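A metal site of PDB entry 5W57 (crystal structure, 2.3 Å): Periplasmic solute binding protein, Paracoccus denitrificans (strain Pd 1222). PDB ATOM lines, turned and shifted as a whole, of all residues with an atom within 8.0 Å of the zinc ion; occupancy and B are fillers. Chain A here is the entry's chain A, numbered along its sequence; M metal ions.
Residues that only touch the zinc ion: Ala 183 (3.98 Å) and Val 201 (3.6 Å). Within 4 Å of the zinc ion: His 38, His 115, His 181, Ala 183, Val 201 and Asp 256.
The zinc ion is bound by OD1 of Asp 256, 2.0 Å away. NE2 of His 38 binds the zinc ion (2.1 Å). A ring nitrogen (NE2) of His 115 binds the zinc ion, at 2.2 Å. NE2 of His 181 binds the zinc ion (2.3 Å). The zinc ion has four donor atoms within binding distance.
The side-chain carboxylate (OD1) of Asp 113 is in hydrogen-bond range of a ring nitrogen (ND1) of His 115, at 2.5 Å. N of His 38 lies within hydrogen-bond range of OD1 of Asp 36. The side-chain hydroxyl (OG) of Ser 202 sits at hydrogen-bond distance from a ring nitrogen (ND1) of His 38 (3.3 Å). The backbone carbonyl oxygen (O) of Val 201 lies close to a ring nitrogen (NE2) of His 115. OD2 of Asp 256 sits close to OG of Ser 255, 3.5 Å away. The backbone carbonyl oxygen (O) of Val 201 sits close to a ring nitrogen (NE2) of His 38 (3.4 Å). A ring nitrogen (ND1) of His 181 is in hydrogen-bond range of the side-chain carboxylate of Glu 230 (2.6 Å).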
ATOM      1  N   ASP A  36       1.679   2.650 -27.648  1.00  0.00           N
ATOM      2  CA  ASP A  36       2.334   3.124 -26.434  1.00  0.00           C
ATOM      3  C   ASP A  36       1.847   4.543 -26.157  1.00  0.00           C
ATOM      4  O   ASP A  36       2.041   5.448 -26.972  1.00  0.00           O
ATOM      5  CB  ASP A  36       3.851   3.043 -26.563  1.00  0.00           C
ATOM      6  CG  ASP A  36       4.591   3.719 -25.423  1.00  0.00           C
ATOM      7  OD1 ASP A  36       3.990   3.977 -24.364  1.00  0.00           O
ATOM      8  OD2 ASP A  36       5.811   3.931 -25.562  1.00  0.00           O
ATOM      9  N   THR A  37       1.202   4.723 -24.997  1.00  0.00           N
ATOM     10  CA  THR A  37       0.658   6.013 -24.576  1.00  0.00           C
ATOM     11  C   THR A  37       1.732   6.940 -24.039  1.00  0.00           C
ATOM     12  O   THR A  37       1.552   8.171 -24.073  1.00  0.00           O
ATOM     13  CB  THR A  37      -0.447   5.804 -23.528  1.00  0.00           C
ATOM     14  OG1 THR A  37      -1.459   4.939 -24.069  1.00  0.00           O
ATOM     15  CG2 THR A  37      -1.092   7.119 -23.132  1.00  0.00           C
ATOM     16  N   HIS A  38       2.860   6.395 -23.574  1.00  0.00           N
ATOM     17  CA  HIS A  38       3.938   7.237 -23.056  1.00  0.00           C
ATOM     18  C   HIS A  38       4.470   8.206 -24.106  1.00  0.00           C
ATOM     19  O   HIS A  38       4.934   9.299 -23.767  1.00  0.00           O
ATOM     20  CB  HIS A  38       5.112   6.377 -22.565  1.00  0.00           C
ATOM     21  CG  HIS A  38       4.815   5.563 -21.343  1.00  0.00           C
ATOM     22  ND1 HIS A  38       4.603   6.125 -20.102  1.00  0.00           N
ATOM     23  CD2 HIS A  38       4.738   4.221 -21.171  1.00  0.00           C
ATOM     24  CE1 HIS A  38       4.396   5.164 -19.220  1.00  0.00           C
ATOM     25  NE2 HIS A  38       4.476   4.002 -19.834  1.00  0.00           N
ATOM     26  N   PHE A  63       0.140   9.718 -16.971  1.00  0.00           N
ATOM     27  CA  PHE A  63       0.310   8.712 -18.009  1.00  0.00           C
ATOM     28  C   PHE A  63       0.167   9.330 -19.383  1.00  0.00           C
ATOM     29  O   PHE A  63       1.010   9.123 -20.268  1.00  0.00           O
ATOM     30  CB  PHE A  63      -0.711   7.580 -17.810  1.00  0.00           C
ATOM     31  CG  PHE A  63      -0.523   6.413 -18.745  1.00  0.00           C
ATOM     32  CD1 PHE A  63       0.725   5.834 -18.917  1.00  0.00           C
ATOM     33  CD2 PHE A  63      -1.605   5.877 -19.429  1.00  0.00           C
ATOM     34  CE1 PHE A  63       0.884   4.745 -19.767  1.00  0.00           C
ATOM     35  CE2 PHE A  63      -1.452   4.792 -20.275  1.00  0.00           C
ATOM     36  CZ  PHE A  63      -0.200   4.222 -20.449  1.00  0.00           C
ATOM     37  N   ASP A 113       3.722   6.055  -9.977  1.00  0.00           N
ATOM     38  CA  ASP A 113       3.665   5.026 -11.003  1.00  0.00           C
ATOM     39  C   ASP A 113       2.227   4.953 -11.524  1.00  0.00           C
ATOM     40  O   ASP A 113       1.312   4.663 -10.735  1.00  0.00           O
ATOM     41  CB  ASP A 113       4.111   3.699 -10.414  1.00  0.00           C
ATOM     42  CG  ASP A 113       4.437   2.667 -11.464  1.00  0.00           C
ATOM     43  OD1 ASP A 113       3.952   2.774 -12.611  1.00  0.00           O
ATOM     44  OD2 ASP A 113       5.182   1.731 -11.116  1.00  0.00           O
ATOM     45  N   PRO A 114       1.983   5.238 -12.795  1.00  0.00           N
ATOM     46  CA  PRO A 114       0.602   5.292 -13.289  1.00  0.00           C
ATOM     47  C   PRO A 114      -0.026   3.943 -13.634  1.00  0.00           C
ATOM     48  O   PRO A 114      -1.220   3.910 -13.933  1.00  0.00           O
ATOM     49  CB  PRO A 114       0.713   6.165 -14.548  1.00  0.00           C
ATOM     50  CG  PRO A 114       2.103   5.951 -15.023  1.00  0.00           C
ATOM     51  CD  PRO A 114       2.950   5.708 -13.795  1.00  0.00           C
ATOM     52  N   HIS A 115       0.742   2.843 -13.628  1.00  0.00           N
ATOM     53  CA  HIS A 115       0.221   1.568 -14.119  1.00  0.00           C
ATOM     54  C   HIS A 115      -0.627   0.870 -13.066  1.00  0.00           C
ATOM     55  O   HIS A 115      -0.372  -0.297 -12.739  1.00  0.00           O
ATOM     56  CB  HIS A 115       1.365   0.646 -14.540  1.00  0.00           C
ATOM     57  CG  HIS A 115       2.384   1.304 -15.421  1.00  0.00           C
ATOM     58  ND1 HIS A 115       3.466   1.985 -14.914  1.00  0.00           N
ATOM     59  CD2 HIS A 115       2.480   1.379 -16.770  1.00  0.00           C
ATOM     60  CE1 HIS A 115       4.183   2.461 -15.921  1.00  0.00           C
ATOM     61  NE2 HIS A 115       3.615   2.104 -17.056  1.00  0.00           N
ATOM     62  N   TRP A 117      -3.604  -0.302 -13.121  1.00  0.00           N
ATOM     63  CA  TRP A 117      -4.464  -1.382 -13.632  1.00  0.00           C
ATOM     64  C   TRP A 117      -3.825  -2.768 -13.525  1.00  0.00           C
ATOM     65  O   TRP A 117      -4.558  -3.765 -13.498  1.00  0.00           O
ATOM     66  CB  TRP A 117      -4.830  -1.127 -15.100  1.00  0.00           C
ATOM     67  CG  TRP A 117      -3.646  -1.089 -16.029  1.00  0.00           C
ATOM     68  CD1 TRP A 117      -3.031  -2.155 -16.636  1.00  0.00           C
ATOM     69  CD2 TRP A 117      -2.912   0.078 -16.441  1.00  0.00           C
ATOM     70  NE1 TRP A 117      -1.973  -1.721 -17.408  1.00  0.00           N
ATOM     71  CE2 TRP A 117      -1.884  -0.348 -17.307  1.00  0.00           C
ATOM     72  CE3 TRP A 117      -3.047   1.446 -16.169  1.00  0.00           C
ATOM     73  CZ2 TRP A 117      -0.992   0.540 -17.892  1.00  0.00           C
ATOM     74  CZ3 TRP A 117      -2.152   2.320 -16.757  1.00  0.00           C
ATOM     75  CH2 TRP A 117      -1.141   1.862 -17.600  1.00  0.00           C
ATOM     76  N   HIS A 181       9.758  -2.638 -20.067  1.00  0.00           N
ATOM     77  CA  HIS A 181       9.868  -1.428 -19.253  1.00  0.00           C
ATOM     78  C   HIS A 181       9.197  -1.657 -17.899  1.00  0.00           C
ATOM     79  O   HIS A 181       8.459  -2.633 -17.708  1.00  0.00           O
ATOM     80  CB  HIS A 181       9.330  -0.187 -20.026  1.00  0.00           C
ATOM     81  CG  HIS A 181       7.829  -0.090 -20.116  1.00  0.00           C
ATOM     82  ND1 HIS A 181       7.079  -0.805 -21.030  1.00  0.00           N
ATOM     83  CD2 HIS A 181       6.951   0.762 -19.518  1.00  0.00           C
ATOM     84  CE1 HIS A 181       5.806  -0.478 -20.926  1.00  0.00           C
ATOM     85  NE2 HIS A 181       5.700   0.478 -20.022  1.00  0.00           N
ATOM     86  N   ASN A 182       9.516  -0.792 -16.944  1.00  0.00           N
ATOM     87  CA  ASN A 182       9.153  -0.971 -15.534  1.00  0.00           C
ATOM     88  C   ASN A 182       7.670  -0.630 -15.331  1.00  0.00           C
ATOM     89  O   ASN A 182       7.306   0.382 -14.732  1.00  0.00           O
ATOM     90  CB  ASN A 182      10.065  -0.111 -14.653  1.00  0.00           C
ATOM     91  CG  ASN A 182      10.041  -0.523 -13.188  1.00  0.00           C
ATOM     92  OD1 ASN A 182       9.357  -1.475 -12.814  1.00  0.00           O
ATOM     93  ND2 ASN A 182      10.784   0.208 -12.354  1.00  0.00           N
ATOM     94  N   ALA A 183       6.824  -1.522 -15.831  1.00  0.00           N
ATOM     95  CA  ALA A 183       5.401  -1.273 -15.980  1.00  0.00           C
ATOM     96  C   ALA A 183       4.528  -2.161 -15.103  1.00  0.00           C
ATOM     97  O   ALA A 183       3.305  -1.980 -15.090  1.00  0.00           O
ATOM     98  CB  ALA A 183       4.991  -1.425 -17.449  1.00  0.00           C
ATOM     99  N   PHE A 184       5.117  -3.098 -14.363  1.00  0.00           N
ATOM    100  CA  PHE A 184       4.378  -4.145 -13.661  1.00  0.00           C
ATOM    101  C   PHE A 184       4.526  -4.047 -12.145  1.00  0.00           C
ATOM    102  O   PHE A 184       4.298  -5.020 -11.432  1.00  0.00           O
ATOM    103  CB  PHE A 184       4.839  -5.521 -14.162  1.00  0.00           C
ATOM    104  CG  PHE A 184       4.437  -5.831 -15.583  1.00  0.00           C
ATOM    105  CD1 PHE A 184       3.196  -6.409 -15.864  1.00  0.00           C
ATOM    106  CD2 PHE A 184       5.306  -5.580 -16.647  1.00  0.00           C
ATOM    107  CE1 PHE A 184       2.824  -6.715 -17.171  1.00  0.00           C
ATOM    108  CE2 PHE A 184       4.945  -5.882 -17.962  1.00  0.00           C
ATOM    109  CZ  PHE A 184       3.720  -6.452 -18.229  1.00  0.00           C
ATOM    110  N   GLY A 200      12.659   2.511 -17.809  1.00  0.00           N
ATOM    111  CA  GLY A 200      12.038   2.925 -16.568  1.00  0.00           C
ATOM    112  C   GLY A 200      10.517   2.851 -16.615  1.00  0.00           C
ATOM    113  O   GLY A 200       9.922   2.120 -17.419  1.00  0.00           O
ATOM    114  N   VAL A 201       9.886   3.626 -15.730  1.00  0.00           N
ATOM    115  CA  VAL A 201       8.423   3.662 -15.641  1.00  0.00           C
ATOM    116  C   VAL A 201       7.805   4.144 -16.944  1.00  0.00           C
ATOM    117  O   VAL A 201       6.699   3.709 -17.313  1.00  0.00           O
ATOM    118  CB  VAL A 201       8.010   4.543 -14.451  1.00  0.00           C
ATOM    119  CG1 VAL A 201       6.490   4.803 -14.458  1.00  0.00           C
ATOM    120  CG2 VAL A 201       8.436   3.899 -13.142  1.00  0.00           C
ATOM    121  N   SER A 202       8.481   5.036 -17.658  1.00  0.00           N
ATOM    122  CA  SER A 202       8.023   5.493 -18.967  1.00  0.00           C
ATOM    123  C   SER A 202       8.999   5.066 -20.053  1.00  0.00           C
ATOM    124  O   SER A 202      10.188   4.886 -19.810  1.00  0.00           O
ATOM    125  CB  SER A 202       7.862   7.009 -18.988  1.00  0.00           C
ATOM    126  OG  SER A 202       7.577   7.445 -20.308  1.00  0.00           O
ATOM    127  N   THR A 203       8.480   4.935 -21.273  1.00  0.00           N
ATOM    128  CA  THR A 203       9.301   4.540 -22.409  1.00  0.00           C
ATOM    129  C   THR A 203       9.848   5.728 -23.188  1.00  0.00           C
ATOM    130  O   THR A 203      10.431   5.519 -24.257  1.00  0.00           O
ATOM    131  CB  THR A 203       8.506   3.626 -23.349  1.00  0.00           C
ATOM    132  OG1 THR A 203       7.266   4.250 -23.694  1.00  0.00           O
ATOM    133  CG2 THR A 203       8.228   2.280 -22.693  1.00  0.00           C
ATOM    134  N   GLU A 230       7.326  -7.117 -24.703  1.00  0.00           N
ATOM    135  CA  GLU A 230       6.037  -6.498 -24.488  1.00  0.00           C
ATOM    136  C   GLU A 230       5.417  -6.171 -25.834  1.00  0.00           C
ATOM    137  O   GLU A 230       6.132  -5.960 -26.829  1.00  0.00           O
ATOM    138  CB  GLU A 230       6.139  -5.213 -23.653  1.00  0.00           C
ATOM    139  CG  GLU A 230       6.234  -5.409 -22.151  1.00  0.00           C
ATOM    140  CD  GLU A 230       6.663  -4.125 -21.473  1.00  0.00           C
ATOM    141  OE1 GLU A 230       6.246  -3.052 -21.960  1.00  0.00           O
ATOM    142  OE2 GLU A 230       7.424  -4.174 -20.469  1.00  0.00           O
ATOM    143  N   ILE A 232       4.005  -3.513 -26.818  1.00  0.00           N
ATOM    144  CA  ILE A 232       4.096  -2.117 -27.242  1.00  0.00           C
ATOM    145  C   ILE A 232       5.523  -1.701 -27.590  1.00  0.00           C
ATOM    146  O   ILE A 232       5.739  -0.555 -27.992  1.00  0.00           O
ATOM    147  CB  ILE A 232       3.539  -1.162 -26.180  1.00  0.00           C
ATOM    148  CG1 ILE A 232       4.366  -1.280 -24.895  1.00  0.00           C
ATOM    149  CG2 ILE A 232       2.074  -1.436 -25.908  1.00  0.00           C
ATOM    150  CD1 ILE A 232       4.284  -0.101 -23.997  1.00  0.00           C
ATOM    151  N   SER A 255       1.477  -4.916 -21.386  1.00  0.00           N
ATOM    152  CA  SER A 255       1.742  -3.936 -20.338  1.00  0.00           C
ATOM    153  C   SER A 255       0.742  -2.782 -20.386  1.00  0.00           C
ATOM    154  O   SER A 255      -0.121  -2.668 -19.504  1.00  0.00           O
ATOM    155  CB  SER A 255       3.172  -3.398 -20.462  1.00  0.00           C
ATOM    156  OG  SER A 255       3.381  -2.778 -21.717  1.00  0.00           O
ATOM    157  N   ASP A 256       0.852  -1.939 -21.414  1.00  0.00           N
ATOM    158  CA  ASP A 256       0.160  -0.657 -21.452  1.00  0.00           C
ATOM    159  C   ASP A 256      -0.941  -0.621 -22.511  1.00  0.00           C
ATOM    160  O   ASP A 256      -1.513   0.437 -22.743  1.00  0.00           O
ATOM    161  CB  ASP A 256       1.154   0.474 -21.743  1.00  0.00           C
ATOM    162  CG  ASP A 256       2.161   0.670 -20.630  1.00  0.00           C
ATOM    163  OD1 ASP A 256       2.904   1.700 -20.688  1.00  0.00           O
ATOM    164  OD2 ASP A 256       2.207  -0.190 -19.713  1.00  0.00           O
ATOM    165  N   ALA A 257      -1.220  -1.743 -23.177  1.00  0.00           N
ATOM    166  CA  ALA A 257      -2.207  -1.758 -24.245  1.00  0.00           C
ATOM    167  C   ALA A 257      -2.742  -3.169 -24.414  1.00  0.00           C
ATOM    168  O   ALA A 257      -2.039  -4.158 -24.174  1.00  0.00           O
ATOM    169  CB  ALA A 257      -1.627  -1.259 -25.572  1.00  0.00           C
HETATM  170 ZN    ZN M   1       4.188   2.049 -19.212  1.00  0.00          ZN
